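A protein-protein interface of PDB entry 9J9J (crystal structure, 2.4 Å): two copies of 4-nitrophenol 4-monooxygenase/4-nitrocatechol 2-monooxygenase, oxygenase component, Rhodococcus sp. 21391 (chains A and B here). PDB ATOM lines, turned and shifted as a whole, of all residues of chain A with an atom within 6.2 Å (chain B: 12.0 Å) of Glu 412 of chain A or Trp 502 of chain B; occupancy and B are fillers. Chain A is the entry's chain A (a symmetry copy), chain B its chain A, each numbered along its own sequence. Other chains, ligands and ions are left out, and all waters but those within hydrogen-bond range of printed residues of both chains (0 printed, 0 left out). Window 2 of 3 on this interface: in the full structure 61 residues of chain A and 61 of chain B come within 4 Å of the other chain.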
ATOM      1  N   GLY A 407     -13.510   1.095 -23.940  1.00  0.00           N
ATOM      2  CA  GLY A 407     -14.850   1.532 -24.261  1.00  0.00           C
ATOM      3  C   GLY A 407     -15.850   0.425 -24.002  1.00  0.00           C
ATOM      4  O   GLY A 407     -16.878   0.651 -23.377  1.00  0.00           O
ATOM      5  N   PRO A 408     -15.629  -0.787 -24.534  1.00  0.00           N
ATOM      6  CA  PRO A 408     -16.514  -1.902 -24.225  1.00  0.00           C
ATOM      7  C   PRO A 408     -16.563  -2.158 -22.728  1.00  0.00           C
ATOM      8  O   PRO A 408     -17.583  -2.613 -22.231  1.00  0.00           O
ATOM      9  CB  PRO A 408     -15.926  -3.082 -25.025  1.00  0.00           C
ATOM     10  CG  PRO A 408     -15.251  -2.419 -26.188  1.00  0.00           C
ATOM     11  CD  PRO A 408     -14.676  -1.108 -25.602  1.00  0.00           C
ATOM     12  N   LYS A 409     -15.497  -1.793 -22.010  1.00  0.00           N
ATOM     13  CA  LYS A 409     -15.459  -1.998 -20.571  1.00  0.00           C
ATOM     14  C   LYS A 409     -16.399  -1.021 -19.871  1.00  0.00           C
ATOM     15  O   LYS A 409     -17.000  -1.379 -18.860  1.00  0.00           O
ATOM     16  CB  LYS A 409     -14.027  -1.949 -20.031  1.00  0.00           C
ATOM     17  CG  LYS A 409     -13.117  -3.065 -20.532  1.00  0.00           C
ATOM     18  CD  LYS A 409     -13.005  -4.267 -19.602  1.00  0.00           C
ATOM     19  CE  LYS A 409     -12.430  -5.535 -20.202  1.00  0.00           C
ATOM     20  NZ  LYS A 409     -11.477  -5.218 -21.263  1.00  0.00           N
ATOM     21  N   LEU A 410     -16.506   0.205 -20.408  1.00  0.00           N
ATOM     22  CA  LEU A 410     -17.437   1.213 -19.902  1.00  0.00           C
ATOM     23  C   LEU A 410     -18.874   0.814 -20.174  1.00  0.00           C
ATOM     24  O   LEU A 410     -19.743   0.958 -19.322  1.00  0.00           O
ATOM     25  CB  LEU A 410     -17.161   2.584 -20.500  1.00  0.00           C
ATOM     26  CG  LEU A 410     -16.020   3.334 -19.824  1.00  0.00           C
ATOM     27  CD1 LEU A 410     -15.533   4.412 -20.742  1.00  0.00           C
ATOM     28  CD2 LEU A 410     -16.462   3.902 -18.486  1.00  0.00           C
ATOM     29  N   GLU A 411     -19.118   0.309 -21.372  1.00  0.00           N
ATOM     30  CA  GLU A 411     -20.458  -0.086 -21.743  1.00  0.00           C
ATOM     31  C   GLU A 411     -20.914  -1.159 -20.778  1.00  0.00           C
ATOM     32  O   GLU A 411     -22.105  -1.286 -20.517  1.00  0.00           O
ATOM     33  CB  GLU A 411     -20.507  -0.626 -23.172  1.00  0.00           C
ATOM     34  CG  GLU A 411     -20.169   0.438 -24.208  1.00  0.00           C
ATOM     35  CD  GLU A 411     -20.375  -0.006 -25.641  1.00  0.00           C
ATOM     36  OE1 GLU A 411     -19.794  -1.026 -26.022  1.00  0.00           O
ATOM     37  OE2 GLU A 411     -21.068   0.687 -26.387  1.00  0.00           O
ATOM     38  N   GLU A 412     -19.949  -1.943 -20.301  1.00  0.00           N
ATOM     39  CA  GLU A 412     -20.209  -3.018 -19.355  1.00  0.00           C
ATOM     40  C   GLU A 412     -20.420  -2.427 -17.972  1.00  0.00           C
ATOM     41  O   GLU A 412     -21.397  -2.712 -17.304  1.00  0.00           O
ATOM     42  CB  GLU A 412     -18.999  -3.961 -19.321  1.00  0.00           C
ATOM     43  CG  GLU A 412     -19.252  -5.270 -18.592  1.00  0.00           C
ATOM     44  CD  GLU A 412     -18.046  -6.129 -18.258  1.00  0.00           C
ATOM     45  OE1 GLU A 412     -16.868  -5.846 -18.630  1.00  0.00           O
ATOM     46  OE2 GLU A 412     -18.355  -7.128 -17.565  1.00  0.00           O
ATOM     47  N   ALA A 413     -19.484  -1.590 -17.543  1.00  0.00           N
ATOM     48  CA  ALA A 413     -19.532  -1.051 -16.202  1.00  0.00           C
ATOM     49  C   ALA A 413     -20.732  -0.134 -15.949  1.00  0.00           C
ATOM     50  O   ALA A 413     -21.206  -0.101 -14.826  1.00  0.00           O
ATOM     51  CB  ALA A 413     -18.265  -0.306 -15.963  1.00  0.00           C
ATOM     52  N   LEU A 414     -21.158   0.682 -16.930  1.00  0.00           N
ATOM     53  CA  LEU A 414     -22.128   1.735 -16.671  1.00  0.00           C
ATOM     54  C   LEU A 414     -23.523   1.387 -17.162  1.00  0.00           C
ATOM     55  O   LEU A 414     -24.377   2.267 -17.128  1.00  0.00           O
ATOM     56  CB  LEU A 414     -21.670   3.027 -17.337  1.00  0.00           C
ATOM     57  CG  LEU A 414     -20.318   3.545 -16.866  1.00  0.00           C
ATOM     58  CD1 LEU A 414     -20.034   4.945 -17.353  1.00  0.00           C
ATOM     59  CD2 LEU A 414     -20.309   3.481 -15.356  1.00  0.00           C
ATOM     60  N   ARG A 415     -23.765   0.154 -17.632  1.00  0.00           N
ATOM     61  CA  ARG A 415     -25.092  -0.211 -18.106  1.00  0.00           C
ATOM     62  C   ARG A 415     -26.041  -0.457 -16.943  1.00  0.00           C
ATOM     63  O   ARG A 415     -25.625  -0.672 -15.819  1.00  0.00           O
ATOM     64  CB  ARG A 415     -25.172  -1.498 -18.925  1.00  0.00           C
ATOM     65  CG  ARG A 415     -24.884  -2.731 -18.095  1.00  0.00           C
ATOM     66  CD  ARG A 415     -24.754  -3.965 -18.960  1.00  0.00           C
ATOM     67  NE  ARG A 415     -23.800  -4.841 -18.275  1.00  0.00           N
ATOM     68  CZ  ARG A 415     -24.081  -6.007 -17.750  1.00  0.00           C
ATOM     69  NH1 ARG A 415     -25.289  -6.504 -17.875  1.00  0.00           N
ATOM     70  NH2 ARG A 415     -23.149  -6.687 -17.121  1.00  0.00           N
ATOM     71  N   ALA A 421     -25.350   1.465 -21.482  1.00  0.00           N
ATOM     72  CA  ALA A 421     -24.542   2.493 -20.871  1.00  0.00           C
ATOM     73  C   ALA A 421     -24.720   3.809 -21.602  1.00  0.00           C
ATOM     74  O   ALA A 421     -24.808   4.858 -20.967  1.00  0.00           O
ATOM     75  CB  ALA A 421     -23.120   2.089 -20.928  1.00  0.00           C
ATOM     76  N   LEU B 489     -36.069   0.322 -25.538  1.00  0.00           N
ATOM     77  CA  LEU B 489     -34.791   0.608 -24.896  1.00  0.00           C
ATOM     78  C   LEU B 489     -34.172  -0.654 -24.307  1.00  0.00           C
ATOM     79  O   LEU B 489     -32.961  -0.820 -24.380  1.00  0.00           O
ATOM     80  CB  LEU B 489     -34.984   1.627 -23.777  1.00  0.00           C
ATOM     81  CG  LEU B 489     -35.141   3.078 -24.216  1.00  0.00           C
ATOM     82  CD1 LEU B 489     -35.720   3.919 -23.099  1.00  0.00           C
ATOM     83  CD2 LEU B 489     -33.772   3.563 -24.631  1.00  0.00           C
ATOM     84  N   ALA B 490     -35.002  -1.472 -23.640  1.00  0.00           N
ATOM     85  CA  ALA B 490     -34.559  -2.712 -23.026  1.00  0.00           C
ATOM     86  C   ALA B 490     -34.039  -3.665 -24.099  1.00  0.00           C
ATOM     87  O   ALA B 490     -33.057  -4.381 -23.879  1.00  0.00           O
ATOM     88  CB  ALA B 490     -35.682  -3.331 -22.210  1.00  0.00           C
ATOM     89  N   ALA B 491     -34.696  -3.630 -25.263  1.00  0.00           N
ATOM     90  CA  ALA B 491     -34.266  -4.404 -26.412  1.00  0.00           C
ATOM     91  C   ALA B 491     -32.859  -4.008 -26.850  1.00  0.00           C
ATOM     92  O   ALA B 491     -32.031  -4.882 -27.065  1.00  0.00           O
ATOM     93  CB  ALA B 491     -35.262  -4.240 -27.541  1.00  0.00           C
ATOM     94  N   ARG B 492     -32.574  -2.707 -27.005  1.00  0.00           N
ATOM     95  CA  ARG B 492     -31.250  -2.297 -27.454  1.00  0.00           C
ATOM     96  C   ARG B 492     -30.197  -2.768 -26.449  1.00  0.00           C
ATOM     97  O   ARG B 492     -29.153  -3.290 -26.826  1.00  0.00           O
ATOM     98  CB  ARG B 492     -31.106  -0.786 -27.671  1.00  0.00           C
ATOM     99  CG  ARG B 492     -29.646  -0.368 -27.878  1.00  0.00           C
ATOM    100  CD  ARG B 492     -29.359   1.131 -28.002  1.00  0.00           C
ATOM    101  NE  ARG B 492     -30.183   1.697 -29.072  1.00  0.00           N
ATOM    102  CZ  ARG B 492     -31.349   2.291 -28.883  1.00  0.00           C
ATOM    103  NH1 ARG B 492     -31.641   2.865 -27.736  1.00  0.00           N
ATOM    104  NH2 ARG B 492     -32.203   2.367 -29.881  1.00  0.00           N
ATOM    105  N   ALA B 493     -30.471  -2.561 -25.159  1.00  0.00           N
ATOM    106  CA  ALA B 493     -29.544  -2.935 -24.108  1.00  0.00           C
ATOM    107  C   ALA B 493     -29.199  -4.418 -24.217  1.00  0.00           C
ATOM    108  O   ALA B 493     -28.029  -4.794 -24.146  1.00  0.00           O
ATOM    109  CB  ALA B 493     -30.155  -2.625 -22.763  1.00  0.00           C
ATOM    110  N   ALA B 494     -30.240  -5.252 -24.340  1.00  0.00           N
ATOM    111  CA  ALA B 494     -30.053  -6.694 -24.332  1.00  0.00           C
ATOM    112  C   ALA B 494     -29.206  -7.078 -25.534  1.00  0.00           C
ATOM    113  O   ALA B 494     -28.281  -7.880 -25.409  1.00  0.00           O
ATOM    114  CB  ALA B 494     -31.380  -7.416 -24.341  1.00  0.00           C
ATOM    115  N   GLU B 495     -29.497  -6.450 -26.678  1.00  0.00           N
ATOM    116  CA  GLU B 495     -28.733  -6.730 -27.877  1.00  0.00           C
ATOM    117  C   GLU B 495     -27.279  -6.311 -27.697  1.00  0.00           C
ATOM    118  O   GLU B 495     -26.387  -7.019 -28.146  1.00  0.00           O
ATOM    119  CB  GLU B 495     -29.404  -6.121 -29.103  1.00  0.00           C
ATOM    120  CG  GLU B 495     -30.769  -6.749 -29.394  1.00  0.00           C
ATOM    121  CD  GLU B 495     -30.880  -8.271 -29.377  1.00  0.00           C
ATOM    122  OE1 GLU B 495     -29.926  -8.945 -29.813  1.00  0.00           O
ATOM    123  OE2 GLU B 495     -31.948  -8.781 -28.972  1.00  0.00           O
ATOM    124  N   VAL B 496     -27.022  -5.185 -27.027  1.00  0.00           N
ATOM    125  CA  VAL B 496     -25.646  -4.745 -26.821  1.00  0.00           C
ATOM    126  C   VAL B 496     -24.908  -5.751 -25.932  1.00  0.00           C
ATOM    127  O   VAL B 496     -23.713  -5.939 -26.093  1.00  0.00           O
ATOM    128  CB  VAL B 496     -25.607  -3.310 -26.254  1.00  0.00           C
ATOM    129  CG1 VAL B 496     -24.242  -2.948 -25.673  1.00  0.00           C
ATOM    130  CG2 VAL B 496     -26.034  -2.281 -27.294  1.00  0.00           C
ATOM    131  N   GLU B 497     -25.620  -6.397 -24.995  1.00  0.00           N
ATOM    132  CA  GLU B 497     -25.065  -7.460 -24.164  1.00  0.00           C
ATOM    133  C   GLU B 497     -24.732  -8.678 -25.024  1.00  0.00           C
ATOM    134  O   GLU B 497     -23.639  -9.229 -24.907  1.00  0.00           O
ATOM    135  CB  GLU B 497     -25.988  -7.920 -23.029  1.00  0.00           C
ATOM    136  CG  GLU B 497     -25.845  -7.120 -21.736  1.00  0.00           C
ATOM    137  CD  GLU B 497     -26.928  -7.333 -20.690  1.00  0.00           C
ATOM    138  OE1 GLU B 497     -27.196  -8.522 -20.432  1.00  0.00           O
ATOM    139  OE2 GLU B 497     -27.482  -6.349 -20.129  1.00  0.00           O
ATOM    140  N   LYS B 498     -25.675  -9.082 -25.887  1.00  0.00           N
ATOM    141  CA  LYS B 498     -25.515 -10.279 -26.704  1.00  0.00           C
ATOM    142  C   LYS B 498     -24.445 -10.086 -27.785  1.00  0.00           C
ATOM    143  O   LYS B 498     -23.877 -11.069 -28.243  1.00  0.00           O
ATOM    144  CB  LYS B 498     -26.849 -10.739 -27.311  1.00  0.00           C
ATOM    145  CG  LYS B 498     -27.816 -11.390 -26.317  1.00  0.00           C
ATOM    146  CD  LYS B 498     -29.281 -11.414 -26.755  1.00  0.00           C
ATOM    147  CE  LYS B 498     -30.177 -12.046 -25.728  1.00  0.00           C
ATOM    148  NZ  LYS B 498     -31.594 -11.888 -26.055  1.00  0.00           N
ATOM    149  N   ASN B 499     -24.148  -8.838 -28.181  1.00  0.00           N
ATOM    150  CA  ASN B 499     -23.182  -8.578 -29.244  1.00  0.00           C
ATOM    151  C   ASN B 499     -21.801  -8.261 -28.661  1.00  0.00           C
ATOM    152  O   ASN B 499     -20.987  -7.631 -29.332  1.00  0.00           O
ATOM    153  CB  ASN B 499     -23.664  -7.471 -30.189  1.00  0.00           C
ATOM    154  CG  ASN B 499     -24.661  -7.955 -31.223  1.00  0.00           C
ATOM    155  OD1 ASN B 499     -24.328  -8.787 -32.075  1.00  0.00           O
ATOM    156  ND2 ASN B 499     -25.883  -7.446 -31.187  1.00  0.00           N
ATOM    157  N   SER B 500     -21.535  -8.678 -27.415  1.00  0.00           N
ATOM    158  CA  SER B 500     -20.241  -8.467 -26.775  1.00  0.00           C
ATOM    159  C   SER B 500     -19.930  -9.676 -25.896  1.00  0.00           C
ATOM    160  O   SER B 500     -20.732 -10.609 -25.853  1.00  0.00           O
ATOM    161  CB  SER B 500     -20.238  -7.185 -25.979  1.00  0.00           C
ATOM    162  OG  SER B 500     -21.338  -7.160 -25.081  1.00  0.00           O
ATOM    163  N   ASN B 501     -18.777  -9.674 -25.205  1.00  0.00           N
ATOM    164  CA  ASN B 501     -18.513 -10.703 -24.200  1.00  0.00           C
ATOM    165  C   ASN B 501     -17.844 -10.093 -22.971  1.00  0.00           C
ATOM    166  O   ASN B 501     -16.807  -9.442 -23.076  1.00  0.00           O
ATOM    167  CB  ASN B 501     -17.778 -11.920 -24.765  1.00  0.00           C
ATOM    168  CG  ASN B 501     -18.702 -13.093 -25.038  1.00  0.00           C
ATOM    169  OD1 ASN B 501     -19.859 -13.121 -24.594  1.00  0.00           O
ATOM    170  ND2 ASN B 501     -18.205 -14.090 -25.754  1.00  0.00           N
ATOM    171  N   TRP B 502     -18.448 -10.390 -21.808  1.00  0.00           N
ATOM    172  CA  TRP B 502     -18.334  -9.600 -20.591  1.00  0.00           C
ATOM    173  C   TRP B 502     -18.300 -10.526 -19.354  1.00  0.00           C
ATOM    174  O   TRP B 502     -17.203 -10.732 -18.789  1.00  0.00           O
ATOM    175  CB  TRP B 502     -19.526  -8.625 -20.508  1.00  0.00           C
ATOM    176  CG  TRP B 502     -19.508  -7.420 -21.422  1.00  0.00           C
ATOM    177  CD1 TRP B 502     -18.453  -6.877 -22.101  1.00  0.00           C
ATOM    178  CD2 TRP B 502     -20.631  -6.544 -21.683  1.00  0.00           C
ATOM    179  NE1 TRP B 502     -18.844  -5.756 -22.789  1.00  0.00           N
ATOM    180  CE2 TRP B 502     -20.171  -5.519 -22.544  1.00  0.00           C
ATOM    181  CE3 TRP B 502     -21.974  -6.526 -21.274  1.00  0.00           C
ATOM    182  CZ2 TRP B 502     -21.006  -4.502 -23.003  1.00  0.00           C
ATOM    183  CZ3 TRP B 502     -22.793  -5.513 -21.724  1.00  0.00           C
ATOM    184  CH2 TRP B 502     -22.314  -4.513 -22.573  1.00  0.00           C
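No position is printed for both chains. Of the 5 pairs that touch across the chains among the printed residues, none has its exchanged pair printed and touching as well.
The backbone carbonyl oxygen (O) of Glu 497 of chain B lies within hydrogen-bond range of the side-chain hydroxyl (OG) of Ser 500 of chain B (3.1 Å). O of Glu 412 of chain A sits at hydrogen-bond distance from NE of Arg 415 of chain A (3.4 Å).
Of chain A, only Pro 408, Glu 411, Glu 412 and Arg 415 come within 4 Å of Trp 502 of chain B. No residue of chain B comes within 4 Å of Ala 413 of chain A. No residue of chain B comes within 4 Å of Leu 414 of chain A. Of the printed residues of chain A, Glu 497 of chain B touches Arg 415 (3.1 Å). The nearest residue of chain A that does not touch Trp 502 of chain B is Lys 409 of chain A (5.2 Å).
Among the printed residues, pairs that only touch across the chains: Glu 412 of chain A with Trp 502 of chain B (3.5 Å), Arg 415 of chain A with Trp 502 of chain B (3.7 Å) and Glu 411 of chain A with Trp 502 of chain B (3.8 Å).
OE2 of Glu 497 of chain B is in salt-bridge range of NH1 of Arg 415 of chain A (3.1 Å). The backbone carbonyl oxygen (O) of Pro 408 of chain A is in hydrogen-bond range of the indole nitrogen (NE1) of Trp 502 of chain B, 3.4 Å away.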
